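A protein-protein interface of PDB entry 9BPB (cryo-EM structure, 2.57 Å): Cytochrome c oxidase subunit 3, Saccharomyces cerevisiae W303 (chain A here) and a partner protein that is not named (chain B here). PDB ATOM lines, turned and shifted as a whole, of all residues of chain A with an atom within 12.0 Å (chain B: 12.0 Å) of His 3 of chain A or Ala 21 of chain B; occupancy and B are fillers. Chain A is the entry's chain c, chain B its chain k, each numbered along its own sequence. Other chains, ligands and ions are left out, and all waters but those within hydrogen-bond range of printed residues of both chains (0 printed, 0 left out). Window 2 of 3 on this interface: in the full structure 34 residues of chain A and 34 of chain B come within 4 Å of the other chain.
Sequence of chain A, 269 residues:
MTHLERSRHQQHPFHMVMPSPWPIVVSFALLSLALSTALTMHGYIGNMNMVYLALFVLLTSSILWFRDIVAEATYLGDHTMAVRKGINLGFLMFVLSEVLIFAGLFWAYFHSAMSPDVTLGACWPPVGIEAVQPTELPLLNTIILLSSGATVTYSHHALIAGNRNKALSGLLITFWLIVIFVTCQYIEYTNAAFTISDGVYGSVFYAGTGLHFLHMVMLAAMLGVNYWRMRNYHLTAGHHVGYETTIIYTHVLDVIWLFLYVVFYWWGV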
ATOM      1  N   MET A   1      22.813 -14.150 -23.534  1.00  0.00           N
ATOM      2  CA  MET A   1      24.207 -14.408 -23.875  1.00  0.00           C
ATOM      3  C   MET A   1      24.334 -14.934 -25.301  1.00  0.00           C
ATOM      4  O   MET A   1      23.662 -15.891 -25.683  1.00  0.00           O
ATOM      5  CB  MET A   1      24.825 -15.399 -22.891  1.00  0.00           C
ATOM      6  CG  MET A   1      26.338 -15.330 -22.810  1.00  0.00           C
ATOM      7  SD  MET A   1      27.019 -16.491 -21.616  1.00  0.00           S
ATOM      8  CE  MET A   1      28.438 -15.581 -21.024  1.00  0.00           C
ATOM      9  N   THR A   2      25.185 -14.277 -26.092  1.00  0.00           N
ATOM     10  CA  THR A   2      25.358 -14.657 -27.513  1.00  0.00           C
ATOM     11  C   THR A   2      26.065 -15.997 -27.607  1.00  0.00           C
ATOM     12  O   THR A   2      26.832 -16.314 -26.692  1.00  0.00           O
ATOM     13  CB  THR A   2      26.203 -13.629 -28.266  1.00  0.00           C
ATOM     14  OG1 THR A   2      25.688 -12.332 -27.971  1.00  0.00           O
ATOM     15  CG2 THR A   2      26.212 -13.837 -29.764  1.00  0.00           C
ATOM     16  N   HIS A   3      25.778 -16.763 -28.648  1.00  0.00           N
ATOM     17  CA  HIS A   3      26.474 -18.018 -28.914  1.00  0.00           C
ATOM     18  C   HIS A   3      27.977 -17.807 -29.040  1.00  0.00           C
ATOM     19  O   HIS A   3      28.762 -18.673 -28.635  1.00  0.00           O
ATOM     20  CB  HIS A   3      25.932 -18.666 -30.189  1.00  0.00           C
ATOM     21  CG  HIS A   3      24.912 -19.734 -29.946  1.00  0.00           C
ATOM     22  ND1 HIS A   3      25.184 -20.872 -29.218  1.00  0.00           N
ATOM     23  CD2 HIS A   3      23.623 -19.845 -30.348  1.00  0.00           C
ATOM     24  CE1 HIS A   3      24.104 -21.632 -29.173  1.00  0.00           C
ATOM     25  NE2 HIS A   3      23.143 -21.032 -29.851  1.00  0.00           N
ATOM     26  N   LEU A   4      28.395 -16.657 -29.578  1.00  0.00           N
ATOM     27  CA  LEU A   4      29.847 -16.374 -29.741  1.00  0.00           C
ATOM     28  C   LEU A   4      30.497 -16.175 -28.370  1.00  0.00           C
ATOM     29  O   LEU A   4      31.639 -16.624 -28.199  1.00  0.00           O
ATOM     30  CB  LEU A   4      30.043 -15.134 -30.614  1.00  0.00           C
ATOM     31  CG  LEU A   4      31.494 -14.776 -30.917  1.00  0.00           C
ATOM     32  CD1 LEU A   4      32.007 -15.574 -32.101  1.00  0.00           C
ATOM     33  CD2 LEU A   4      31.644 -13.287 -31.168  1.00  0.00           C
ATOM     34  N   GLU A   5      29.806 -15.520 -27.435  1.00  0.00           N
ATOM     35  CA  GLU A   5      30.398 -15.257 -26.128  1.00  0.00           C
ATOM     36  C   GLU A   5      30.544 -16.533 -25.311  1.00  0.00           C
ATOM     37  O   GLU A   5      31.554 -16.727 -24.626  1.00  0.00           O
ATOM     38  CB  GLU A   5      29.556 -14.229 -25.373  1.00  0.00           C
ATOM     39  CG  GLU A   5      30.068 -13.901 -23.980  1.00  0.00           C
ATOM     40  CD  GLU A   5      31.406 -13.190 -24.001  1.00  0.00           C
ATOM     41  OE1 GLU A   5      31.710 -12.519 -25.009  1.00  0.00           O
ATOM     42  OE2 GLU A   5      32.151 -13.301 -23.007  1.00  0.00           O
ATOM     43  N   ARG A   6      29.539 -17.412 -25.363  1.00  0.00           N
ATOM     44  CA  ARG A   6      29.570 -18.621 -24.546  1.00  0.00           C
ATOM     45  C   ARG A   6      30.728 -19.534 -24.926  1.00  0.00           C
ATOM     46  O   ARG A   6      31.248 -20.263 -24.073  1.00  0.00           O
ATOM     47  CB  ARG A   6      28.242 -19.366 -24.668  1.00  0.00           C
ATOM     48  CG  ARG A   6      28.101 -20.543 -23.718  1.00  0.00           C
ATOM     49  CD  ARG A   6      28.463 -20.146 -22.303  1.00  0.00           C
ATOM     50  NE  ARG A   6      28.412 -21.279 -21.389  1.00  0.00           N
ATOM     51  CZ  ARG A   6      29.469 -21.988 -21.020  1.00  0.00           C
ATOM     52  NH1 ARG A   6      30.677 -21.720 -21.489  1.00  0.00           N
ATOM     53  NH2 ARG A   6      29.313 -22.989 -20.163  1.00  0.00           N
ATOM     54  N   SER A   7      31.152 -19.507 -26.187  1.00  0.00           N
ATOM     55  CA  SER A   7      32.244 -20.350 -26.655  1.00  0.00           C
ATOM     56  C   SER A   7      33.608 -19.852 -26.203  1.00  0.00           C
ATOM     57  O   SER A   7      34.616 -20.507 -26.483  1.00  0.00           O
ATOM     58  CB  SER A   7      32.211 -20.448 -28.181  1.00  0.00           C
ATOM     59  OG  SER A   7      32.534 -19.203 -28.774  1.00  0.00           O
ATOM     60  N   ARG A   8      33.661 -18.713 -25.520  1.00  0.00           N
ATOM     61  CA  ARG A   8      34.895 -18.119 -25.027  1.00  0.00           C
ATOM     62  C   ARG A   8      35.033 -18.401 -23.532  1.00  0.00           C
ATOM     63  O   ARG A   8      35.564 -17.601 -22.762  1.00  0.00           O
ATOM     64  CB  ARG A   8      34.912 -16.623 -25.343  1.00  0.00           C
ATOM     65  CG  ARG A   8      36.191 -15.867 -25.023  1.00  0.00           C
ATOM     66  CD  ARG A   8      36.419 -14.767 -26.043  1.00  0.00           C
ATOM     67  NE  ARG A   8      35.173 -14.103 -26.405  1.00  0.00           N
ATOM     68  CZ  ARG A   8      34.900 -12.831 -26.154  1.00  0.00           C
ATOM     69  NH1 ARG A   8      35.768 -12.045 -25.539  1.00  0.00           N
ATOM     70  NH2 ARG A   8      33.726 -12.333 -26.533  1.00  0.00           N
ATOM     71  N   HIS A   9      34.547 -19.568 -23.112  1.00  0.00           N
ATOM     72  CA  HIS A   9      34.523 -19.964 -21.711  1.00  0.00           C
ATOM     73  C   HIS A   9      34.518 -21.484 -21.646  1.00  0.00           C
ATOM     74  O   HIS A   9      34.275 -22.165 -22.645  1.00  0.00           O
ATOM     75  CB  HIS A   9      33.296 -19.401 -20.979  1.00  0.00           C
ATOM     76  CG  HIS A   9      33.307 -17.911 -20.825  1.00  0.00           C
ATOM     77  ND1 HIS A   9      34.059 -17.266 -19.869  1.00  0.00           N
ATOM     78  CD2 HIS A   9      32.659 -16.940 -21.513  1.00  0.00           C
ATOM     79  CE1 HIS A   9      33.873 -15.961 -19.970  1.00  0.00           C
ATOM     80  NE2 HIS A   9      33.027 -15.738 -20.960  1.00  0.00           N
ATOM     81  N   GLN A  10      34.812 -22.014 -20.458  1.00  0.00           N
ATOM     82  CA  GLN A  10      34.819 -23.490 -20.280  1.00  0.00           C
ATOM     83  C   GLN A  10      33.390 -23.997 -20.440  1.00  0.00           C
ATOM     84  O   GLN A  10      32.461 -23.265 -20.083  1.00  0.00           O
ATOM     85  CB  GLN A  10      35.373 -23.916 -18.921  1.00  0.00           C
ATOM     86  CG  GLN A  10      36.839 -24.309 -18.945  1.00  0.00           C
ATOM     87  CD  GLN A  10      37.264 -24.896 -17.623  1.00  0.00           C
ATOM     88  OE1 GLN A  10      38.209 -24.436 -16.988  1.00  0.00           O
ATOM     89  NE2 GLN A  10      36.565 -25.935 -17.200  1.00  0.00           N
ATOM     90  N   GLN A  11      33.232 -25.204 -20.963  1.00  0.00           N
ATOM     91  CA  GLN A  11      31.891 -25.805 -21.184  1.00  0.00           C
ATOM     92  C   GLN A  11      31.586 -26.741 -20.016  1.00  0.00           C
ATOM     93  O   GLN A  11      30.470 -27.277 -19.968  1.00  0.00           O
ATOM     94  CB  GLN A  11      31.833 -26.549 -22.518  1.00  0.00           C
ATOM     95  CG  GLN A  11      32.342 -25.758 -23.710  1.00  0.00           C
ATOM     96  CD  GLN A  11      31.404 -24.637 -24.077  1.00  0.00           C
ATOM     97  OE1 GLN A  11      30.210 -24.848 -24.271  1.00  0.00           O
ATOM     98  NE2 GLN A  11      31.937 -23.430 -24.157  1.00  0.00           N
ATOM     99  N   LYS B  19      21.460 -17.611 -31.543  1.00  0.00           N
ATOM    100  CA  LYS B  19      22.431 -16.865 -30.699  1.00  0.00           C
ATOM    101  C   LYS B  19      22.050 -16.887 -29.213  1.00  0.00           C
ATOM    102  O   LYS B  19      22.974 -17.003 -28.400  1.00  0.00           O
ATOM    103  CB  LYS B  19      22.573 -15.438 -31.238  1.00  0.00           C
ATOM    104  CG  LYS B  19      23.042 -15.329 -32.683  1.00  0.00           C
ATOM    105  CD  LYS B  19      24.459 -14.818 -32.837  1.00  0.00           C
ATOM    106  CE  LYS B  19      25.522 -15.834 -32.477  1.00  0.00           C
ATOM    107  NZ  LYS B  19      25.566 -16.961 -33.436  1.00  0.00           N
ATOM    108  N   PRO B  20      20.765 -16.840 -28.797  1.00  0.00           N
ATOM    109  CA  PRO B  20      20.419 -16.683 -27.376  1.00  0.00           C
ATOM    110  C   PRO B  20      21.109 -17.669 -26.449  1.00  0.00           C
ATOM    111  O   PRO B  20      21.118 -17.435 -25.235  1.00  0.00           O
ATOM    112  CB  PRO B  20      18.900 -16.887 -27.362  1.00  0.00           C
ATOM    113  CG  PRO B  20      18.460 -16.519 -28.731  1.00  0.00           C
ATOM    114  CD  PRO B  20      19.569 -16.948 -29.649  1.00  0.00           C
ATOM    115  N   ALA B  21      21.669 -18.761 -26.976  1.00  0.00           N
ATOM    116  CA  ALA B  21      22.297 -19.793 -26.155  1.00  0.00           C
ATOM    117  C   ALA B  21      21.288 -20.388 -25.184  1.00  0.00           C
ATOM    118  O   ALA B  21      20.544 -21.309 -25.538  1.00  0.00           O
ATOM    119  CB  ALA B  21      23.512 -19.242 -25.403  1.00  0.00           C
ATOM    120  N   PHE B  22      21.258 -19.875 -23.957  1.00  0.00           N
ATOM    121  CA  PHE B  22      20.316 -20.370 -22.966  1.00  0.00           C
ATOM    122  C   PHE B  22      18.891 -19.981 -23.343  1.00  0.00           C
ATOM    123  O   PHE B  22      18.660 -19.092 -24.164  1.00  0.00           O
ATOM    124  CB  PHE B  22      20.655 -19.816 -21.584  1.00  0.00           C
ATOM    125  CG  PHE B  22      22.111 -19.900 -21.243  1.00  0.00           C
ATOM    126  CD1 PHE B  22      22.699 -21.117 -20.964  1.00  0.00           C
ATOM    127  CD2 PHE B  22      22.891 -18.759 -21.200  1.00  0.00           C
ATOM    128  CE1 PHE B  22      24.038 -21.198 -20.655  1.00  0.00           C
ATOM    129  CE2 PHE B  22      24.231 -18.834 -20.888  1.00  0.00           C
ATOM    130  CZ  PHE B  22      24.805 -20.055 -20.615  1.00  0.00           C
ATOM    131  N   GLY B  23      17.928 -20.658 -22.726  1.00  0.00           N
ATOM    132  CA  GLY B  23      16.533 -20.374 -22.960  1.00  0.00           C
ATOM    133  C   GLY B  23      16.063 -19.176 -22.164  1.00  0.00           C
ATOM    134  O   GLY B  23      16.863 -18.438 -21.581  1.00  0.00           O
ATOM    135  N   PRO B  24      14.751 -18.954 -22.132  1.00  0.00           N
ATOM    136  CA  PRO B  24      14.204 -17.835 -21.357  1.00  0.00           C
ATOM    137  C   PRO B  24      14.530 -17.984 -19.884  1.00  0.00           C
ATOM    138  O   PRO B  24      14.532 -19.105 -19.353  1.00  0.00           O
ATOM    139  CB  PRO B  24      12.691 -17.935 -21.608  1.00  0.00           C
ATOM    140  CG  PRO B  24      12.467 -19.355 -22.004  1.00  0.00           C
ATOM    141  CD  PRO B  24      13.694 -19.760 -22.762  1.00  0.00           C
ATOM    142  N   PRO B  25      14.827 -16.884 -19.193  1.00  0.00           N
ATOM    143  CA  PRO B  25      15.130 -16.974 -17.759  1.00  0.00           C
ATOM    144  C   PRO B  25      13.964 -17.563 -16.981  1.00  0.00           C
ATOM    145  O   PRO B  25      12.798 -17.277 -17.262  1.00  0.00           O
ATOM    146  CB  PRO B  25      15.401 -15.518 -17.357  1.00  0.00           C
ATOM    147  CG  PRO B  25      14.858 -14.685 -18.474  1.00  0.00           C
ATOM    148  CD  PRO B  25      14.972 -15.514 -19.708  1.00  0.00           C
ATOM    149  N   ASP B  26      14.295 -18.398 -15.997  1.00  0.00           N
ATOM    150  CA  ASP B  26      13.265 -19.084 -15.224  1.00  0.00           C
ATOM    151  C   ASP B  26      12.427 -18.097 -14.418  1.00  0.00           C
ATOM    152  O   ASP B  26      11.194 -18.187 -14.401  1.00  0.00           O
ATOM    153  CB  ASP B  26      13.908 -20.123 -14.306  1.00  0.00           C
ATOM    154  CG  ASP B  26      12.957 -21.246 -13.939  1.00  0.00           C
ATOM    155  OD1 ASP B  26      11.784 -20.958 -13.626  1.00  0.00           O
ATOM    156  OD2 ASP B  26      13.386 -22.418 -13.963  1.00  0.00           O
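The backbone carbonyl oxygen (O) of Arg 6 of chain A lies within hydrogen-bond range of the side-chain amide nitrogen (NE2) of Gln 11 of chain A.
NH1 of Arg 6 of chain A sits at hydrogen-bond distance from O of Gln 10 of chain A, at 2.7 Å.
Of the 11 printed residues of chain A, 4 touch a printed residue of chain B.
Hydrophobic or aromatic side chains of chain A within 4 Å of the printed part of chain B: Met 1 and His 3.
Of the 8 printed residues of chain B, 4 touch a printed residue of chain A.
Among the printed residues, 8 pairs touch across the chains.
Among the printed residues, no Asp or Glu carboxylate lies within 4 Å of a Lys or Arg side-chain nitrogen of the other chain.
The backbone NH (N) of His 3 of chain A is in hydrogen-bond range of the backbone carbonyl oxygen (O) of Lys 19 of chain B, at 2.8 Å.
The backbone carbonyl oxygen (O) of Lys 19 of chain B sits close to the backbone carbonyl oxygen (O) of Met 1 of chain A.
O of Met 1 of chain A sits close to O of Pro 20 of chain B, at 3.0 Å.
His 3 of chain A touches just these residues of chain B: Lys 19 (2.8 Å) and Ala 21 (3.9 Å).
Of chain A, only Met 1 (3.4 Å) and His 3 (3.9 Å) come within 4 Å of Ala 21 of chain B.
Met 1 of chain A touches just these residues of chain B: Lys 19, Pro 20, Ala 21 and Phe 22.
Of chain B, only Lys 19 comes within 4 Å of Thr 2 of chain A.
No residue of chain B comes within 4 Å of Leu 4 of chain A.
No residue of chain B comes within 4 Å of Ser 7 of chain A.
Lys 19 of chain B touches three residues of chain A.
Printed residues of chain B within 4 Å of Arg 6 of chain A: Phe 22.
Pro 24 of chain B touches none of the printed residues of chain A.
The nearest residue of chain B that does not touch His 3 of chain A is Pro 20 of chain B (4.4 Å).
The nearest residue of chain A that does not touch Ala 21 of chain B is Thr 2 of chain A (4.6 Å).
Met 1 of chain A touches Ala 21 of chain B (O to CB, 3.4 Å).
Phe 22 of chain B touches Met 1 of chain A.
Lys 19 of chain B touches Thr 2 of chain A (O to C, 3.3 Å).
NE2 of His 3 of chain A touches N of Ala 21 of chain B, 3.9 Å away.
NE of Arg 6 of chain A touches CZ of Phe 22 of chain B (3.9 Å).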
